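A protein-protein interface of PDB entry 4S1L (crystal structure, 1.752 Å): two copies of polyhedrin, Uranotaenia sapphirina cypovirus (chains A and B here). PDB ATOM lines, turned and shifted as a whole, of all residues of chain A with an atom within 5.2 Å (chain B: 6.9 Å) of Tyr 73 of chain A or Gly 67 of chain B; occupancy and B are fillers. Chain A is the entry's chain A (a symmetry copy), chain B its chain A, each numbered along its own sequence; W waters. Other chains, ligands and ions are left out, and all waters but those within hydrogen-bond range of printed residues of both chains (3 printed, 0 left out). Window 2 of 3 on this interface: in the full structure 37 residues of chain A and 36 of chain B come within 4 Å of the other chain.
N of Glu 72 of chain A lies within hydrogen-bond range of OE1 of Gln 69 of chain B (3.4 Å).
The side-chain amide oxygen (OE1) of Gln 69 of chain B sits at hydrogen-bond distance from the backbone NH (N) of Tyr 73 of chain A, at 3.0 Å.
The side-chain carboxylate (OD2) of Asp 63 of chain B is in hydrogen-bond range of the side-chain amide nitrogen (NE2) of Gln 69 of chain B (3.1 Å).
The side-chain carboxylate of Asp 63 of chain B lies within hydrogen-bond range of the indole nitrogen of Trp 210 of chain B (2.9 Å).
N of Ser 71 of chain A lies within hydrogen-bond range of OE2 of Glu 74 of chain A.
OE1 of Gln 69 of chain B touches CB of Ser 71 of chain A, 3.2 Å away.
Tyr 73 of chain A touches Ile 64 of chain B.
Gly 67 of chain B touches Tyr 73 of chain A (O to CE2, 3.8 Å).
Tyr 73 of chain A touches Trp 210 of chain B.
Of the printed residues of chain B, Glu 72 of chain A touches Gln 69.
Tyr 73 of chain A touches just these residues of chain B: Ile 64, Gly 67, Gln 69 and Trp 210.
Gly 67 of chain B touches just one residue of chain A: Tyr 73 (3.8 Å).
Of the printed residues of chain A, Gln 69 of chain B touches Ser 71, Glu 72 and Tyr 73.
The nearest residue of chain A that does not touch Gly 67 of chain B is Arg 77 of chain A (5.0 Å).
The nearest printed residue of chain B that does not touch Ser 71 of chain A is His 68 of chain B (5.8 Å).
Along chain B the printed residues that touch a printed residue of chain A span positions 64 to 210.
Of the 7 printed residues of chain A, 3 touch a printed residue of chain B.
Hydrophobic or aromatic side chains of chain A that line the printed part of chain B: Tyr 73.
No position is printed for both chains.
Water W1 lies within hydrogen-bond range of the side-chain carboxylate of Glu 72 of chain A and the side-chain amide nitrogen of Gln 69 of chain B.
Water W2 lies within hydrogen-bond range of OG of Ser 71 of chain A, N of Gln 69 of chain B and OE2 of Glu 74 of chain A.
Water W3 bridges N of Glu 72 of chain A (3.0 Å) and OE1 of Gln 69 of chain B (3.4 Å).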
ATOM      1  N   SER A  71      23.885 -11.061  10.060  1.00  0.00           N
ATOM      2  CA  SER A  71      24.795 -10.685  11.144  1.00  0.00           C
ATOM      3  C   SER A  71      24.403 -11.325  12.467  1.00  0.00           C
ATOM      4  O   SER A  71      23.242 -11.704  12.662  1.00  0.00           O
ATOM      5  CB  SER A  71      24.811  -9.179  11.331  1.00  0.00           C
ATOM      6  OG  SER A  71      23.526  -8.765  11.747  1.00  0.00           O
ATOM      7  N   GLU A  72      25.369 -11.422  13.386  1.00  0.00           N
ATOM      8  CA  GLU A  72      25.073 -11.912  14.726  1.00  0.00           C
ATOM      9  C   GLU A  72      23.973 -11.042  15.374  1.00  0.00           C
ATOM     10  O   GLU A  72      23.119 -11.545  16.078  1.00  0.00           O
ATOM     11  CB  GLU A  72      26.331 -11.932  15.598  1.00  0.00           C
ATOM     12  CG  GLU A  72      26.071 -12.559  16.981  1.00  0.00           C
ATOM     13  CD  GLU A  72      27.292 -12.642  17.863  1.00  0.00           C
ATOM     14  OE1 GLU A  72      28.327 -12.046  17.516  1.00  0.00           O
ATOM     15  OE2 GLU A  72      27.201 -13.296  18.917  1.00  0.00           O
ATOM     16  N   TYR A  73      24.011  -9.737  15.138  1.00  0.00           N
ATOM     17  CA  TYR A  73      23.005  -8.829  15.691  1.00  0.00           C
ATOM     18  C   TYR A  73      21.558  -9.217  15.322  1.00  0.00           C
ATOM     19  O   TYR A  73      20.676  -9.294  16.189  1.00  0.00           O
ATOM     20  CB  TYR A  73      23.317  -7.417  15.212  1.00  0.00           C
ATOM     21  CG  TYR A  73      22.291  -6.374  15.535  1.00  0.00           C
ATOM     22  CD1 TYR A  73      22.161  -5.884  16.813  1.00  0.00           C
ATOM     23  CD2 TYR A  73      21.471  -5.860  14.546  1.00  0.00           C
ATOM     24  CE1 TYR A  73      21.212  -4.907  17.114  1.00  0.00           C
ATOM     25  CE2 TYR A  73      20.527  -4.892  14.827  1.00  0.00           C
ATOM     26  CZ  TYR A  73      20.410  -4.416  16.111  1.00  0.00           C
ATOM     27  OH  TYR A  73      19.491  -3.439  16.384  1.00  0.00           O
ATOM     28  N   GLU A  74      21.313  -9.436  14.032  1.00  0.00           N
ATOM     29  CA  GLU A  74      19.989  -9.843  13.556  1.00  0.00           C
ATOM     30  C   GLU A  74      19.601 -11.205  14.109  1.00  0.00           C
ATOM     31  O   GLU A  74      18.448 -11.413  14.498  1.00  0.00           O
ATOM     32  CB  GLU A  74      19.923  -9.943  12.033  1.00  0.00           C
ATOM     33  CG  GLU A  74      20.365  -8.780  11.242  1.00  0.00           C
ATOM     34  CD  GLU A  74      20.548  -9.197   9.779  1.00  0.00           C
ATOM     35  OE1 GLU A  74      19.516  -9.369   9.101  1.00  0.00           O
ATOM     36  OE2 GLU A  74      21.704  -9.408   9.331  1.00  0.00           O
ATOM     37  N   LEU A  75      20.550 -12.142  14.109  1.00  0.00           N
ATOM     38  CA  LEU A  75      20.233 -13.501  14.568  1.00  0.00           C
ATOM     39  C   LEU A  75      19.924 -13.510  16.071  1.00  0.00           C
ATOM     40  O   LEU A  75      18.964 -14.156  16.520  1.00  0.00           O
ATOM     41  CB  LEU A  75      21.381 -14.458  14.253  1.00  0.00           C
ATOM     42  CG  LEU A  75      21.641 -14.683  12.753  1.00  0.00           C
ATOM     43  CD1 LEU A  75      23.023 -15.318  12.547  1.00  0.00           C
ATOM     44  CD2 LEU A  75      20.526 -15.518  12.144  1.00  0.00           C
ATOM     45  N   GLN A  76      20.729 -12.785  16.853  1.00  0.00           N
ATOM     46  CA  GLN A  76      20.521 -12.771  18.300  1.00  0.00           C
ATOM     47  C   GLN A  76      19.187 -12.113  18.625  1.00  0.00           C
ATOM     48  O   GLN A  76      18.495 -12.503  19.570  1.00  0.00           O
ATOM     49  CB  GLN A  76      21.647 -12.031  19.012  1.00  0.00           C
ATOM     50  CG  GLN A  76      21.551 -12.069  20.563  1.00  0.00           C
ATOM     51  CD  GLN A  76      21.646 -13.488  21.082  1.00  0.00           C
ATOM     52  OE1 GLN A  76      22.487 -14.254  20.631  1.00  0.00           O
ATOM     53  NE2 GLN A  76      20.762 -13.856  22.005  1.00  0.00           N
ATOM     54  N   ARG A  77      18.813 -11.131  17.820  1.00  0.00           N
ATOM     55  CA  ARG A  77      17.547 -10.440  18.030  1.00  0.00           C
ATOM     56  C   ARG A  77      16.395 -11.435  17.983  1.00  0.00           C
ATOM     57  O   ARG A  77      15.452 -11.353  18.791  1.00  0.00           O
ATOM     58  CB  ARG A  77      17.356  -9.345  16.984  1.00  0.00           C
ATOM     59  CG  ARG A  77      16.068  -8.534  17.220  1.00  0.00           C
ATOM     60  CD  ARG A  77      15.967  -7.304  16.308  1.00  0.00           C
ATOM     61  NE  ARG A  77      16.163  -7.667  14.904  1.00  0.00           N
ATOM     62  CZ  ARG A  77      16.633  -6.849  13.966  1.00  0.00           C
ATOM     63  NH1 ARG A  77      16.951  -5.593  14.267  1.00  0.00           N
ATOM     64  NH2 ARG A  77      16.786  -7.290  12.721  1.00  0.00           N
ATOM     65  N   TRP B  62      30.204   0.366  19.936  1.00  0.00           N
ATOM     66  CA  TRP B  62      28.808   0.263  19.541  1.00  0.00           C
ATOM     67  C   TRP B  62      28.828   0.136  18.038  1.00  0.00           C
ATOM     68  O   TRP B  62      29.302   1.046  17.348  1.00  0.00           O
ATOM     69  CB  TRP B  62      27.963   1.459  19.972  1.00  0.00           C
ATOM     70  CG  TRP B  62      26.515   1.327  19.509  1.00  0.00           C
ATOM     71  CD1 TRP B  62      25.896   2.033  18.517  1.00  0.00           C
ATOM     72  CD2 TRP B  62      25.531   0.412  20.027  1.00  0.00           C
ATOM     73  NE1 TRP B  62      24.585   1.611  18.383  1.00  0.00           N
ATOM     74  CE2 TRP B  62      24.337   0.620  19.298  1.00  0.00           C
ATOM     75  CE3 TRP B  62      25.551  -0.564  21.031  1.00  0.00           C
ATOM     76  CZ2 TRP B  62      23.175  -0.101  19.550  1.00  0.00           C
ATOM     77  CZ3 TRP B  62      24.397  -1.282  21.282  1.00  0.00           C
ATOM     78  CH2 TRP B  62      23.223  -1.044  20.548  1.00  0.00           C
ATOM     79  N   ASP B  63      28.355  -1.005  17.541  1.00  0.00           N
ATOM     80  CA  ASP B  63      28.570  -1.373  16.143  1.00  0.00           C
ATOM     81  C   ASP B  63      27.321  -1.427  15.268  1.00  0.00           C
ATOM     82  O   ASP B  63      27.323  -2.084  14.226  1.00  0.00           O
ATOM     83  CB  ASP B  63      29.305  -2.733  16.080  1.00  0.00           C
ATOM     84  CG  ASP B  63      28.655  -3.820  16.944  1.00  0.00           C
ATOM     85  OD1 ASP B  63      27.819  -3.516  17.808  1.00  0.00           O
ATOM     86  OD2 ASP B  63      28.994  -5.007  16.752  1.00  0.00           O
ATOM     87  N   ILE B  64      26.281  -0.702  15.653  1.00  0.00           N
ATOM     88  CA  ILE B  64      25.040  -0.659  14.878  1.00  0.00           C
ATOM     89  C   ILE B  64      24.932   0.687  14.183  1.00  0.00           C
ATOM     90  O   ILE B  64      25.106   1.740  14.795  1.00  0.00           O
ATOM     91  CB  ILE B  64      23.805  -0.924  15.781  1.00  0.00           C
ATOM     92  CG1 ILE B  64      24.021  -2.206  16.597  1.00  0.00           C
ATOM     93  CG2 ILE B  64      22.524  -1.054  14.973  1.00  0.00           C
ATOM     94  CD1 ILE B  64      24.519  -3.411  15.788  1.00  0.00           C
ATOM     95  N   ASP B  65      24.670   0.640  12.886  1.00  0.00           N
ATOM     96  CA  ASP B  65      24.591   1.846  12.066  1.00  0.00           C
ATOM     97  C   ASP B  65      23.356   1.733  11.181  1.00  0.00           C
ATOM     98  O   ASP B  65      23.320   0.908  10.286  1.00  0.00           O
ATOM     99  CB  ASP B  65      25.861   2.012  11.233  1.00  0.00           C
ATOM    100  CG  ASP B  65      25.865   3.291  10.419  1.00  0.00           C
ATOM    101  OD1 ASP B  65      25.196   4.267  10.818  1.00  0.00           O
ATOM    102  OD2 ASP B  65      26.559   3.317   9.384  1.00  0.00           O
ATOM    103  N   ASN B  66      22.349   2.554  11.476  1.00  0.00           N
ATOM    104  CA  ASN B  66      21.085   2.537  10.749  1.00  0.00           C
ATOM    105  C   ASN B  66      20.512   1.118  10.640  1.00  0.00           C
ATOM    106  O   ASN B  66      20.170   0.651   9.551  1.00  0.00           O
ATOM    107  CB  ASN B  66      21.278   3.167   9.363  1.00  0.00           C
ATOM    108  CG  ASN B  66      21.637   4.658   9.440  1.00  0.00           C
ATOM    109  OD1 ASN B  66      20.949   5.445  10.094  1.00  0.00           O
ATOM    110  ND2 ASN B  66      22.726   5.041   8.782  1.00  0.00           N
ATOM    111  N   GLY B  67      20.425   0.434  11.774  1.00  0.00           N
ATOM    112  CA  GLY B  67      19.846  -0.896  11.828  1.00  0.00           C
ATOM    113  C   GLY B  67      20.694  -2.066  11.358  1.00  0.00           C
ATOM    114  O   GLY B  67      20.217  -3.203  11.412  1.00  0.00           O
ATOM    115  N   HIS B  68      21.921  -1.820  10.891  1.00  0.00           N
ATOM    116  CA  HIS B  68      22.771  -2.923  10.419  1.00  0.00           C
ATOM    117  C   HIS B  68      24.082  -3.003  11.216  1.00  0.00           C
ATOM    118  O   HIS B  68      24.580  -2.002  11.717  1.00  0.00           O
ATOM    119  CB  HIS B  68      23.042  -2.786   8.908  1.00  0.00           C
ATOM    120  CG  HIS B  68      24.154  -1.844   8.558  1.00  0.00           C
ATOM    121  ND1 HIS B  68      23.933  -0.623   7.950  1.00  0.00           N
ATOM    122  CD2 HIS B  68      25.500  -1.959   8.685  1.00  0.00           C
ATOM    123  CE1 HIS B  68      25.091  -0.018   7.745  1.00  0.00           C
ATOM    124  NE2 HIS B  68      26.059  -0.807   8.185  1.00  0.00           N
ATOM    125  N   GLN B  69      24.635  -4.204  11.347  1.00  0.00           N
ATOM    126  CA  GLN B  69      25.862  -4.371  12.119  1.00  0.00           C
ATOM    127  C   GLN B  69      27.088  -4.045  11.282  1.00  0.00           C
ATOM    128  O   GLN B  69      27.239  -4.543  10.166  1.00  0.00           O
ATOM    129  CB  GLN B  69      25.972  -5.796  12.654  1.00  0.00           C
ATOM    130  CG  GLN B  69      27.144  -5.963  13.601  1.00  0.00           C
ATOM    131  CD  GLN B  69      27.164  -7.319  14.271  1.00  0.00           C
ATOM    132  OE1 GLN B  69      26.312  -8.174  13.999  1.00  0.00           O
ATOM    133  NE2 GLN B  69      28.134  -7.528  15.162  1.00  0.00           N
ATOM    134  N   GLN B 209      24.699  -9.587  23.660  1.00  0.00           N
ATOM    135  CA  GLN B 209      23.371  -9.040  23.424  1.00  0.00           C
ATOM    136  C   GLN B 209      23.460  -7.527  23.300  1.00  0.00           C
ATOM    137  O   GLN B 209      24.343  -6.899  23.877  1.00  0.00           O
ATOM    138  CB  GLN B 209      22.413  -9.458  24.534  1.00  0.00           C
ATOM    139  CG  GLN B 209      21.914 -10.912  24.460  1.00  0.00           C
ATOM    140  CD  GLN B 209      21.124 -11.294  25.683  1.00  0.00           C
ATOM    141  OE1 GLN B 209      21.609 -11.157  26.789  1.00  0.00           O
ATOM    142  NE2 GLN B 209      19.889 -11.731  25.497  1.00  0.00           N
ATOM    143  N   TRP B 210      22.555  -6.978  22.492  1.00  0.00           N
ATOM    144  CA  TRP B 210      22.419  -5.543  22.253  1.00  0.00           C
ATOM    145  C   TRP B 210      21.080  -5.024  22.790  1.00  0.00           C
ATOM    146  O   TRP B 210      20.044  -5.617  22.493  1.00  0.00           O
ATOM    147  CB  TRP B 210      22.461  -5.248  20.753  1.00  0.00           C
ATOM    148  CG  TRP B 210      23.762  -5.489  20.043  1.00  0.00           C
ATOM    149  CD1 TRP B 210      24.636  -4.532  19.631  1.00  0.00           C
ATOM    150  CD2 TRP B 210      24.325  -6.749  19.628  1.00  0.00           C
ATOM    151  NE1 TRP B 210      25.696  -5.099  18.987  1.00  0.00           N
ATOM    152  CE2 TRP B 210      25.536  -6.459  18.963  1.00  0.00           C
ATOM    153  CE3 TRP B 210      23.924  -8.080  19.741  1.00  0.00           C
ATOM    154  CZ2 TRP B 210      26.355  -7.451  18.429  1.00  0.00           C
ATOM    155  CZ3 TRP B 210      24.744  -9.074  19.210  1.00  0.00           C
ATOM    156  CH2 TRP B 210      25.945  -8.750  18.554  1.00  0.00           C
ATOM    157  N   PHE B 211      21.090  -3.882  23.495  1.00  0.00           N
ATOM    158  CA  PHE B 211      19.872  -3.258  24.034  1.00  0.00           C
ATOM    159  C   PHE B 211      19.891  -1.773  23.712  1.00  0.00           C
ATOM    160  O   PHE B 211      20.950  -1.150  23.755  1.00  0.00           O
ATOM    161  CB  PHE B 211      19.776  -3.490  25.555  1.00  0.00           C
ATOM    162  CG  PHE B 211      19.817  -4.941  25.944  1.00  0.00           C
ATOM    163  CD1 PHE B 211      18.667  -5.694  25.967  1.00  0.00           C
ATOM    164  CD2 PHE B 211      21.019  -5.558  26.274  1.00  0.00           C
ATOM    165  CE1 PHE B 211      18.694  -7.043  26.307  1.00  0.00           C
ATOM    166  CE2 PHE B 211      21.044  -6.917  26.623  1.00  0.00           C
ATOM    167  CZ  PHE B 211      19.874  -7.639  26.649  1.00  0.00           C
ATOM    168  N   ASP B 212      18.741  -1.199  23.344  1.00  0.00           N
ATOM    169  CA  ASP B 212      18.712   0.236  23.028  1.00  0.00           C
ATOM    170  C   ASP B 212      18.719   1.107  24.269  1.00  0.00           C
ATOM    171  O   ASP B 212      19.049   2.275  24.192  1.00  0.00           O
ATOM    172  CB  ASP B 212      17.515   0.575  22.159  1.00  0.00           C
ATOM    173  CG  ASP B 212      17.720   0.117  20.732  1.00  0.00           C
ATOM    174  OD1 ASP B 212      18.615   0.668  20.067  1.00  0.00           O
ATOM    175  OD2 ASP B 212      17.027  -0.818  20.308  1.00  0.00           O
HETATM  176  O   HOH W   1      29.165  -9.803  16.481  1.00  0.00           O
HETATM  177  O   HOH W   2      22.880  -6.325  10.435  1.00  0.00           O
HETATM  178  O   HOH W   3      28.131 -10.686  12.639  1.00  0.00           O
